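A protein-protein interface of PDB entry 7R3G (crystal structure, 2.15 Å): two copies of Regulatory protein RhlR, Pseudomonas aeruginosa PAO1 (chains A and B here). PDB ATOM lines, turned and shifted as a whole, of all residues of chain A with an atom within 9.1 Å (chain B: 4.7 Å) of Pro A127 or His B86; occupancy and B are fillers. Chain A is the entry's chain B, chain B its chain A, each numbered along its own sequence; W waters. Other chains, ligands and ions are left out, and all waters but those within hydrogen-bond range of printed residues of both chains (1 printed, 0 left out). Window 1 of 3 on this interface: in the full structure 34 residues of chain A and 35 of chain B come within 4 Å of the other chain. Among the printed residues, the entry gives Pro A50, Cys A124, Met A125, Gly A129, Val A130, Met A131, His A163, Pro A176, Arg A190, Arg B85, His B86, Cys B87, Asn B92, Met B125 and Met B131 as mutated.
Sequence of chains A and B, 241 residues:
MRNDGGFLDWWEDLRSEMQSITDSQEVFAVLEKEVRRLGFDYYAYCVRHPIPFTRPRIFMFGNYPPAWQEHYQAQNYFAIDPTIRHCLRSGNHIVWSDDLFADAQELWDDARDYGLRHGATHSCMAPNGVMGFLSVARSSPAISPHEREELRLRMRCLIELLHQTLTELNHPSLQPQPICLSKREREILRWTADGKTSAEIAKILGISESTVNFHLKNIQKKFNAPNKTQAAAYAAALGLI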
ATOM      1  N   PRO A  50       9.762  17.618  17.875  1.00  0.00           N
ATOM      2  CA  PRO A  50       9.535  18.764  16.981  1.00  0.00           C
ATOM      3  C   PRO A  50       8.993  20.001  17.671  1.00  0.00           C
ATOM      4  O   PRO A  50       9.079  21.092  17.091  1.00  0.00           O
ATOM      5  CB  PRO A  50       8.522  18.215  15.964  1.00  0.00           C
ATOM      6  CG  PRO A  50       7.758  17.200  16.739  1.00  0.00           C
ATOM      7  CD  PRO A  50       8.724  16.580  17.721  1.00  0.00           C
ATOM      8  N   CYS A 124      17.570  10.069  11.196  1.00  0.00           N
ATOM      9  CA  CYS A 124      16.362   9.319  10.892  1.00  0.00           C
ATOM     10  C   CYS A 124      15.186  10.096  11.462  1.00  0.00           C
ATOM     11  O   CYS A 124      15.304  10.760  12.494  1.00  0.00           O
ATOM     12  CB  CYS A 124      16.413   7.899  11.465  1.00  0.00           C
ATOM     13  SG  CYS A 124      16.208   7.793  13.258  1.00  0.00           S
ATOM     14  N   MET A 125      14.057  10.037  10.766  1.00  0.00           N
ATOM     15  CA  MET A 125      12.860  10.761  11.182  1.00  0.00           C
ATOM     16  C   MET A 125      11.709   9.776  11.292  1.00  0.00           C
ATOM     17  O   MET A 125      11.254   9.238  10.279  1.00  0.00           O
ATOM     18  CB  MET A 125      12.515  11.886  10.204  1.00  0.00           C
ATOM     19  CG  MET A 125      11.232  12.624  10.569  1.00  0.00           C
ATOM     20  SD  MET A 125      11.320  14.400  10.271  1.00  0.00           S
ATOM     21  CE  MET A 125       9.693  14.733   9.604  1.00  0.00           C
ATOM     22  N   ALA A 126      11.257   9.527  12.518  1.00  0.00           N
ATOM     23  CA  ALA A 126      10.002   8.825  12.725  1.00  0.00           C
ATOM     24  C   ALA A 126       8.847   9.674  12.195  1.00  0.00           C
ATOM     25  O   ALA A 126       8.889  10.904  12.269  1.00  0.00           O
ATOM     26  CB  ALA A 126       9.792   8.530  14.207  1.00  0.00           C
ATOM     27  N   PRO A 127       7.803   9.044  11.650  1.00  0.00           N
ATOM     28  CA  PRO A 127       6.678   9.837  11.123  1.00  0.00           C
ATOM     29  C   PRO A 127       5.800  10.481  12.193  1.00  0.00           C
ATOM     30  O   PRO A 127       4.682  10.916  11.893  1.00  0.00           O
ATOM     31  CB  PRO A 127       5.887   8.817  10.288  1.00  0.00           C
ATOM     32  CG  PRO A 127       6.297   7.472  10.812  1.00  0.00           C
ATOM     33  CD  PRO A 127       7.716   7.621  11.265  1.00  0.00           C
ATOM     34  N   ASN A 128       6.294  10.567  13.433  1.00  0.00           N
ATOM     35  CA  ASN A 128       5.640  11.321  14.500  1.00  0.00           C
ATOM     36  C   ASN A 128       6.412  12.591  14.853  1.00  0.00           C
ATOM     37  O   ASN A 128       6.298  13.097  15.977  1.00  0.00           O
ATOM     38  CB  ASN A 128       5.468  10.452  15.745  1.00  0.00           C
ATOM     39  CG  ASN A 128       6.795  10.061  16.367  1.00  0.00           C
ATOM     40  OD1 ASN A 128       7.858  10.380  15.838  1.00  0.00           O
ATOM     41  ND2 ASN A 128       6.740   9.366  17.495  1.00  0.00           N
ATOM     42  N   GLY A 129       7.216  13.102  13.921  1.00  0.00           N
ATOM     43  CA  GLY A 129       7.967  14.317  14.134  1.00  0.00           C
ATOM     44  C   GLY A 129       9.274  14.146  14.867  1.00  0.00           C
ATOM     45  O   GLY A 129      10.142  15.023  14.767  1.00  0.00           O
ATOM     46  N   VAL A 130       9.453  13.048  15.599  1.00  0.00           N
ATOM     47  CA  VAL A 130      10.698  12.824  16.325  1.00  0.00           C
ATOM     48  C   VAL A 130      11.818  12.526  15.339  1.00  0.00           C
ATOM     49  O   VAL A 130      11.655  11.725  14.408  1.00  0.00           O
ATOM     50  CB  VAL A 130      10.536  11.681  17.336  1.00  0.00           C
ATOM     51  CG1 VAL A 130      11.865  11.380  18.003  1.00  0.00           C
ATOM     52  CG2 VAL A 130       9.473  12.026  18.367  1.00  0.00           C
ATOM     53  N   MET A 131      12.970  13.157  15.553  1.00  0.00           N
ATOM     54  CA  MET A 131      14.147  12.976  14.715  1.00  0.00           C
ATOM     55  C   MET A 131      15.300  12.451  15.557  1.00  0.00           C
ATOM     56  O   MET A 131      15.556  12.964  16.653  1.00  0.00           O
ATOM     57  CB  MET A 131      14.552  14.290  14.051  1.00  0.00           C
ATOM     58  CG  MET A 131      14.104  14.442  12.616  1.00  0.00           C
ATOM     59  SD  MET A 131      14.847  15.882  11.821  1.00  0.00           S
ATOM     60  CE  MET A 131      15.882  15.073  10.604  1.00  0.00           C
ATOM     61  N   HIS A 163      17.105   3.260  17.682  1.00  0.00           N
ATOM     62  CA  HIS A 163      15.790   3.854  17.904  1.00  0.00           C
ATOM     63  C   HIS A 163      14.741   2.785  18.186  1.00  0.00           C
ATOM     64  O   HIS A 163      13.871   2.972  19.044  1.00  0.00           O
ATOM     65  CB  HIS A 163      15.404   4.702  16.690  1.00  0.00           C
ATOM     66  CG  HIS A 163      13.932   4.925  16.544  1.00  0.00           C
ATOM     67  ND1 HIS A 163      13.151   4.188  15.680  1.00  0.00           N
ATOM     68  CD2 HIS A 163      13.099   5.811  17.140  1.00  0.00           C
ATOM     69  CE1 HIS A 163      11.899   4.604  15.758  1.00  0.00           C
ATOM     70  NE2 HIS A 163      11.842   5.587  16.637  1.00  0.00           N
ATOM     71  N   PRO A 176       6.684  10.592  23.355  1.00  0.00           N
ATOM     72  CA  PRO A 176       6.075  11.923  23.247  1.00  0.00           C
ATOM     73  C   PRO A 176       4.879  12.078  24.174  1.00  0.00           C
ATOM     74  O   PRO A 176       4.213  11.113  24.553  1.00  0.00           O
ATOM     75  CB  PRO A 176       5.654  12.003  21.771  1.00  0.00           C
ATOM     76  CG  PRO A 176       5.657  10.584  21.249  1.00  0.00           C
ATOM     77  CD  PRO A 176       6.228   9.669  22.291  1.00  0.00           C
ATOM     78  N   ARG A 186     -10.437  15.107  15.565  1.00  0.00           N
ATOM     79  CA  ARG A 186      -9.356  15.067  14.587  1.00  0.00           C
ATOM     80  C   ARG A 186      -9.780  15.677  13.257  1.00  0.00           C
ATOM     81  O   ARG A 186      -9.001  16.404  12.629  1.00  0.00           O
ATOM     82  CB  ARG A 186      -8.887  13.624  14.400  1.00  0.00           C
ATOM     83  CG  ARG A 186      -7.751  13.444  13.409  1.00  0.00           C
ATOM     84  CD  ARG A 186      -7.282  11.991  13.378  1.00  0.00           C
ATOM     85  NE  ARG A 186      -6.567  11.618  14.595  1.00  0.00           N
ATOM     86  CZ  ARG A 186      -7.092  10.937  15.606  1.00  0.00           C
ATOM     87  NH1 ARG A 186      -8.350  10.524  15.586  1.00  0.00           N
ATOM     88  NH2 ARG A 186      -6.335  10.663  16.665  1.00  0.00           N
ATOM     89  N   ARG A 190      -8.300  18.999  11.558  1.00  0.00           N
ATOM     90  CA  ARG A 190      -7.754  18.920  10.211  1.00  0.00           C
ATOM     91  C   ARG A 190      -8.320  20.028   9.332  1.00  0.00           C
ATOM     92  O   ARG A 190      -7.568  20.765   8.683  1.00  0.00           O
ATOM     93  CB  ARG A 190      -8.049  17.543   9.618  1.00  0.00           C
ATOM     94  CG  ARG A 190      -7.280  17.261   8.346  1.00  0.00           C
ATOM     95  CD  ARG A 190      -6.967  15.779   8.160  1.00  0.00           C
ATOM     96  NE  ARG A 190      -7.855  14.911   8.921  1.00  0.00           N
ATOM     97  CZ  ARG A 190      -7.512  13.727   9.408  1.00  0.00           C
ATOM     98  NH1 ARG A 190      -6.298  13.230   9.232  1.00  0.00           N
ATOM     99  NH2 ARG A 190      -8.411  13.020  10.085  1.00  0.00           N
ATOM    100  N   ALA A 235      -0.424  19.685  16.215  1.00  0.00           N
ATOM    101  CA  ALA A 235      -0.974  18.450  15.664  1.00  0.00           C
ATOM    102  C   ALA A 235      -0.262  18.071  14.373  1.00  0.00           C
ATOM    103  O   ALA A 235       0.053  16.898  14.150  1.00  0.00           O
ATOM    104  CB  ALA A 235      -2.479  18.595  15.427  1.00  0.00           C
ATOM    105  N   ALA A 236       0.015  19.054  13.517  1.00  0.00           N
ATOM    106  CA  ALA A 236       0.708  18.770  12.266  1.00  0.00           C
ATOM    107  C   ALA A 236       2.109  18.225  12.526  1.00  0.00           C
ATOM    108  O   ALA A 236       2.484  17.171  12.003  1.00  0.00           O
ATOM    109  CB  ALA A 236       0.761  20.027  11.400  1.00  0.00           C
ATOM    110  N   ALA A 237       2.897  18.924  13.349  1.00  0.00           N
ATOM    111  CA  ALA A 237       4.269  18.486  13.597  1.00  0.00           C
ATOM    112  C   ALA A 237       4.321  17.117  14.267  1.00  0.00           C
ATOM    113  O   ALA A 237       5.283  16.367  14.069  1.00  0.00           O
ATOM    114  CB  ALA A 237       5.002  19.518  14.455  1.00  0.00           C
ATOM    115  N   LEU A 238       3.315  16.773  15.062  1.00  0.00           N
ATOM    116  CA  LEU A 238       3.298  15.483  15.738  1.00  0.00           C
ATOM    117  C   LEU A 238       2.763  14.359  14.862  1.00  0.00           C
ATOM    118  O   LEU A 238       2.794  13.198  15.284  1.00  0.00           O
ATOM    119  CB  LEU A 238       2.465  15.584  17.015  1.00  0.00           C
ATOM    120  CG  LEU A 238       3.111  16.377  18.151  1.00  0.00           C
ATOM    121  CD1 LEU A 238       2.083  16.686  19.221  1.00  0.00           C
ATOM    122  CD2 LEU A 238       4.291  15.600  18.724  1.00  0.00           C
ATOM    123  N   GLY A 239       2.289  14.669  13.657  1.00  0.00           N
ATOM    124  CA  GLY A 239       1.705  13.662  12.795  1.00  0.00           C
ATOM    125  C   GLY A 239       0.299  13.260  13.162  1.00  0.00           C
ATOM    126  O   GLY A 239      -0.182  12.228  12.687  1.00  0.00           O
ATOM    127  N   LEU A 240      -0.383  14.051  13.985  1.00  0.00           N
ATOM    128  CA  LEU A 240      -1.688  13.684  14.515  1.00  0.00           C
ATOM    129  C   LEU A 240      -2.846  14.047  13.595  1.00  0.00           C
ATOM    130  O   LEU A 240      -3.966  13.577  13.827  1.00  0.00           O
ATOM    131  CB  LEU A 240      -1.908  14.356  15.873  1.00  0.00           C
ATOM    132  CG  LEU A 240      -0.896  14.023  16.969  1.00  0.00           C
ATOM    133  CD1 LEU A 240      -1.178  14.870  18.201  1.00  0.00           C
ATOM    134  CD2 LEU A 240      -0.915  12.539  17.310  1.00  0.00           C
ATOM    135  N   ILE A 241      -2.619  14.868  12.574  1.00  0.00           N
ATOM    136  CA  ILE A 241      -3.684  15.239  11.646  1.00  0.00           C
ATOM    137  C   ILE A 241      -3.202  15.019  10.215  1.00  0.00           C
ATOM    138  O   ILE A 241      -3.985  15.030   9.264  1.00  0.00           O
ATOM    139  CB  ILE A 241      -4.146  16.696  11.857  1.00  0.00           C
ATOM    140  CG1 ILE A 241      -2.948  17.652  11.869  1.00  0.00           C
ATOM    141  CG2 ILE A 241      -4.932  16.816  13.158  1.00  0.00           C
ATOM    142  CD1 ILE A 241      -3.287  19.074  11.436  1.00  0.00           C
ATOM    143  OXT ILE A 241      -2.009  14.822   9.975  1.00  0.00           O
ATOM    144  N   ARG B  48       3.471  10.544  -0.756  1.00  0.00           N
ATOM    145  CA  ARG B  48       2.415  11.241  -0.031  1.00  0.00           C
ATOM    146  C   ARG B  48       2.982  12.548   0.505  1.00  0.00           C
ATOM    147  O   ARG B  48       3.834  12.543   1.399  1.00  0.00           O
ATOM    148  CB  ARG B  48       1.863  10.378   1.102  1.00  0.00           C
ATOM    149  CG  ARG B  48       0.790  11.063   1.933  1.00  0.00           C
ATOM    150  CD  ARG B  48       0.553  10.330   3.242  1.00  0.00           C
ATOM    151  NE  ARG B  48      -0.635  10.815   3.932  1.00  0.00           N
ATOM    152  CZ  ARG B  48      -0.714  11.977   4.566  1.00  0.00           C
ATOM    153  NH1 ARG B  48       0.311  12.813   4.606  1.00  0.00           N
ATOM    154  NH2 ARG B  48      -1.847  12.306   5.180  1.00  0.00           N
ATOM    155  N   ILE B  84      -0.496   2.876   3.111  1.00  0.00           N
ATOM    156  CA  ILE B  84      -0.033   4.226   2.824  1.00  0.00           C
ATOM    157  C   ILE B  84      -0.563   5.225   3.847  1.00  0.00           C
ATOM    158  O   ILE B  84      -0.680   6.406   3.556  1.00  0.00           O
ATOM    159  CB  ILE B  84      -0.415   4.659   1.393  1.00  0.00           C
ATOM    160  CG1 ILE B  84      -1.930   4.565   1.189  1.00  0.00           C
ATOM    161  CG2 ILE B  84       0.328   3.822   0.375  1.00  0.00           C
ATOM    162  CD1 ILE B  84      -2.447   5.402   0.027  1.00  0.00           C
ATOM    163  N   ARG B  85      -0.902   4.754   5.041  1.00  0.00           N
ATOM    164  CA  ARG B  85      -1.348   5.655   6.091  1.00  0.00           C
ATOM    165  C   ARG B  85      -0.172   6.468   6.618  1.00  0.00           C
ATOM    166  O   ARG B  85       0.963   5.988   6.684  1.00  0.00           O
ATOM    167  CB  ARG B  85      -2.006   4.868   7.223  1.00  0.00           C
ATOM    168  CG  ARG B  85      -3.431   5.314   7.531  1.00  0.00           C
ATOM    169  CD  ARG B  85      -4.184   4.281   8.364  1.00  0.00           C
ATOM    170  NE  ARG B  85      -5.389   3.807   7.693  1.00  0.00           N
ATOM    171  CZ  ARG B  85      -6.034   2.690   8.004  1.00  0.00           C
ATOM    172  NH1 ARG B  85      -5.628   1.908   8.991  1.00  0.00           N
ATOM    173  NH2 ARG B  85      -7.111   2.346   7.303  1.00  0.00           N
ATOM    174  N   HIS B  86      -0.452   7.723   6.972  1.00  0.00           N
ATOM    175  CA  HIS B  86       0.523   8.634   7.571  1.00  0.00           C
ATOM    176  C   HIS B  86       0.625   8.301   9.056  1.00  0.00           C
ATOM    177  O   HIS B  86       0.042   8.959   9.920  1.00  0.00           O
ATOM    178  CB  HIS B  86       0.087  10.076   7.341  1.00  0.00           C
ATOM    179  CG  HIS B  86       1.060  11.105   7.827  1.00  0.00           C
ATOM    180  ND1 HIS B  86       2.125  10.808   8.650  1.00  0.00           N
ATOM    181  CD2 HIS B  86       1.114  12.441   7.611  1.00  0.00           C
ATOM    182  CE1 HIS B  86       2.797  11.915   8.912  1.00  0.00           C
ATOM    183  NE2 HIS B  86       2.205  12.920   8.294  1.00  0.00           N
ATOM    184  N   CYS B  87       1.384   7.249   9.356  1.00  0.00           N
ATOM    185  CA  CYS B  87       1.424   6.719  10.709  1.00  0.00           C
ATOM    186  C   CYS B  87       2.781   6.085  10.971  1.00  0.00           C
ATOM    187  O   CYS B  87       3.625   5.976  10.078  1.00  0.00           O
ATOM    188  CB  CYS B  87       0.300   5.701  10.935  1.00  0.00           C
ATOM    189  SG  CYS B  87       0.774   3.991  10.606  1.00  0.00           S
ATOM    190  N   LEU B  88       2.973   5.663  12.220  1.00  0.00           N
ATOM    191  CA  LEU B  88       4.243   5.132  12.698  1.00  0.00           C
ATOM    192  C   LEU B  88       4.196   3.610  12.677  1.00  0.00           C
ATOM    193  O   LEU B  88       3.322   3.002  13.303  1.00  0.00           O
ATOM    194  CB  LEU B  88       4.542   5.633  14.110  1.00  0.00           C
ATOM    195  N   ASN B  92       9.600   0.836  10.079  1.00  0.00           N
ATOM    196  CA  ASN B  92       9.118   1.442   8.838  1.00  0.00           C
ATOM    197  C   ASN B  92       8.726   0.375   7.824  1.00  0.00           C
ATOM    198  O   ASN B  92       8.879   0.555   6.615  1.00  0.00           O
ATOM    199  CB  ASN B  92      10.163   2.385   8.239  1.00  0.00           C
ATOM    200  CG  ASN B  92      10.491   3.548   9.155  1.00  0.00           C
ATOM    201  OD1 ASN B  92      11.658   3.834   9.412  1.00  0.00           O
ATOM    202  ND2 ASN B  92       9.462   4.228   9.649  1.00  0.00           N
ATOM    203  N   MET B 125      10.354   8.714   5.403  1.00  0.00           N
ATOM    204  CA  MET B 125       9.839  10.075   5.504  1.00  0.00           C
ATOM    205  C   MET B 125      11.022  11.025   5.435  1.00  0.00           C
ATOM    206  O   MET B 125      11.877  11.019   6.326  1.00  0.00           O
ATOM    207  CB  MET B 125       9.041  10.288   6.789  1.00  0.00           C
ATOM    208  CG  MET B 125       8.492  11.706   6.923  1.00  0.00           C
ATOM    209  SD  MET B 125       7.496  11.948   8.402  1.00  0.00           S
ATOM    210  CE  MET B 125       6.879  13.612   8.158  1.00  0.00           C
ATOM    211  N   MET B 131       6.414  11.585   2.459  1.00  0.00           N
ATOM    212  CA  MET B 131       6.591  10.179   2.782  1.00  0.00           C
ATOM    213  C   MET B 131       6.584   9.351   1.506  1.00  0.00           C
ATOM    214  O   MET B 131       5.776   9.591   0.599  1.00  0.00           O
ATOM    215  CB  MET B 131       5.477   9.668   3.699  1.00  0.00           C
ATOM    216  CG  MET B 131       5.619  10.041   5.157  1.00  0.00           C
ATOM    217  SD  MET B 131       4.379   9.199   6.170  1.00  0.00           S
ATOM    218  CE  MET B 131       5.003   7.524   6.148  1.00  0.00           C
HETATM  219  O   HOH W   1      -3.535  14.436   6.747  1.00  0.00           O
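A ring nitrogen (ND1) of His B86 sits at hydrogen-bond distance from the side-chain sulfur (SD) of Met B131 (3.7 Å).
Met B125 touches Met A125. His B86 touches Pro A127. CG of Pro A127 touches O of Cys B87 (3.1 Å). Pro A127 touches Leu B88 (CG to CA, 3.6 Å). Pro A127 touches Met B125.
Water W1 lies within hydrogen-bond range of O of Ile A241 (2.6 Å) and NH2 of Arg B48 (3.1 Å).
Pro A127 touches just these residues of chain B: His B86, Cys B87, Leu B88 and Met B125. His B86 touches one residue of chain A. Of the printed residues of chain A, Leu B88 touches Pro A127 (3.6 Å). Of the printed residues of chain A, Met B125 touches Met A125 (3.4 Å) and Pro A127 (3.5 Å). The nearest residue of chain B that does not touch Pro A127 is Asn B92 (4.1 Å). The nearest residue of chain A that does not touch His B86 is Gly A239 (4.3 Å). The nearest printed residue of chain B that does not touch Met A125 is Asn B92 (5.4 Å).
Of the 9 printed residues of chain B, 4 touch a printed residue of chain A. Hydrophobic or aromatic side chains of chain B that line the printed part of chain A: His B86 and Met B125. Hydrophobic or aromatic side chains of chain A within 4 Å of the printed part of chain B: Met A125 and Pro A127. Among the printed residues, no Asp or Glu carboxylate lies within 4 Å of a Lys or Arg side-chain nitrogen of the other chain.
Met B125 touches its own counterpart, Met A125. Positions printed for both chains: 125 and 131.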
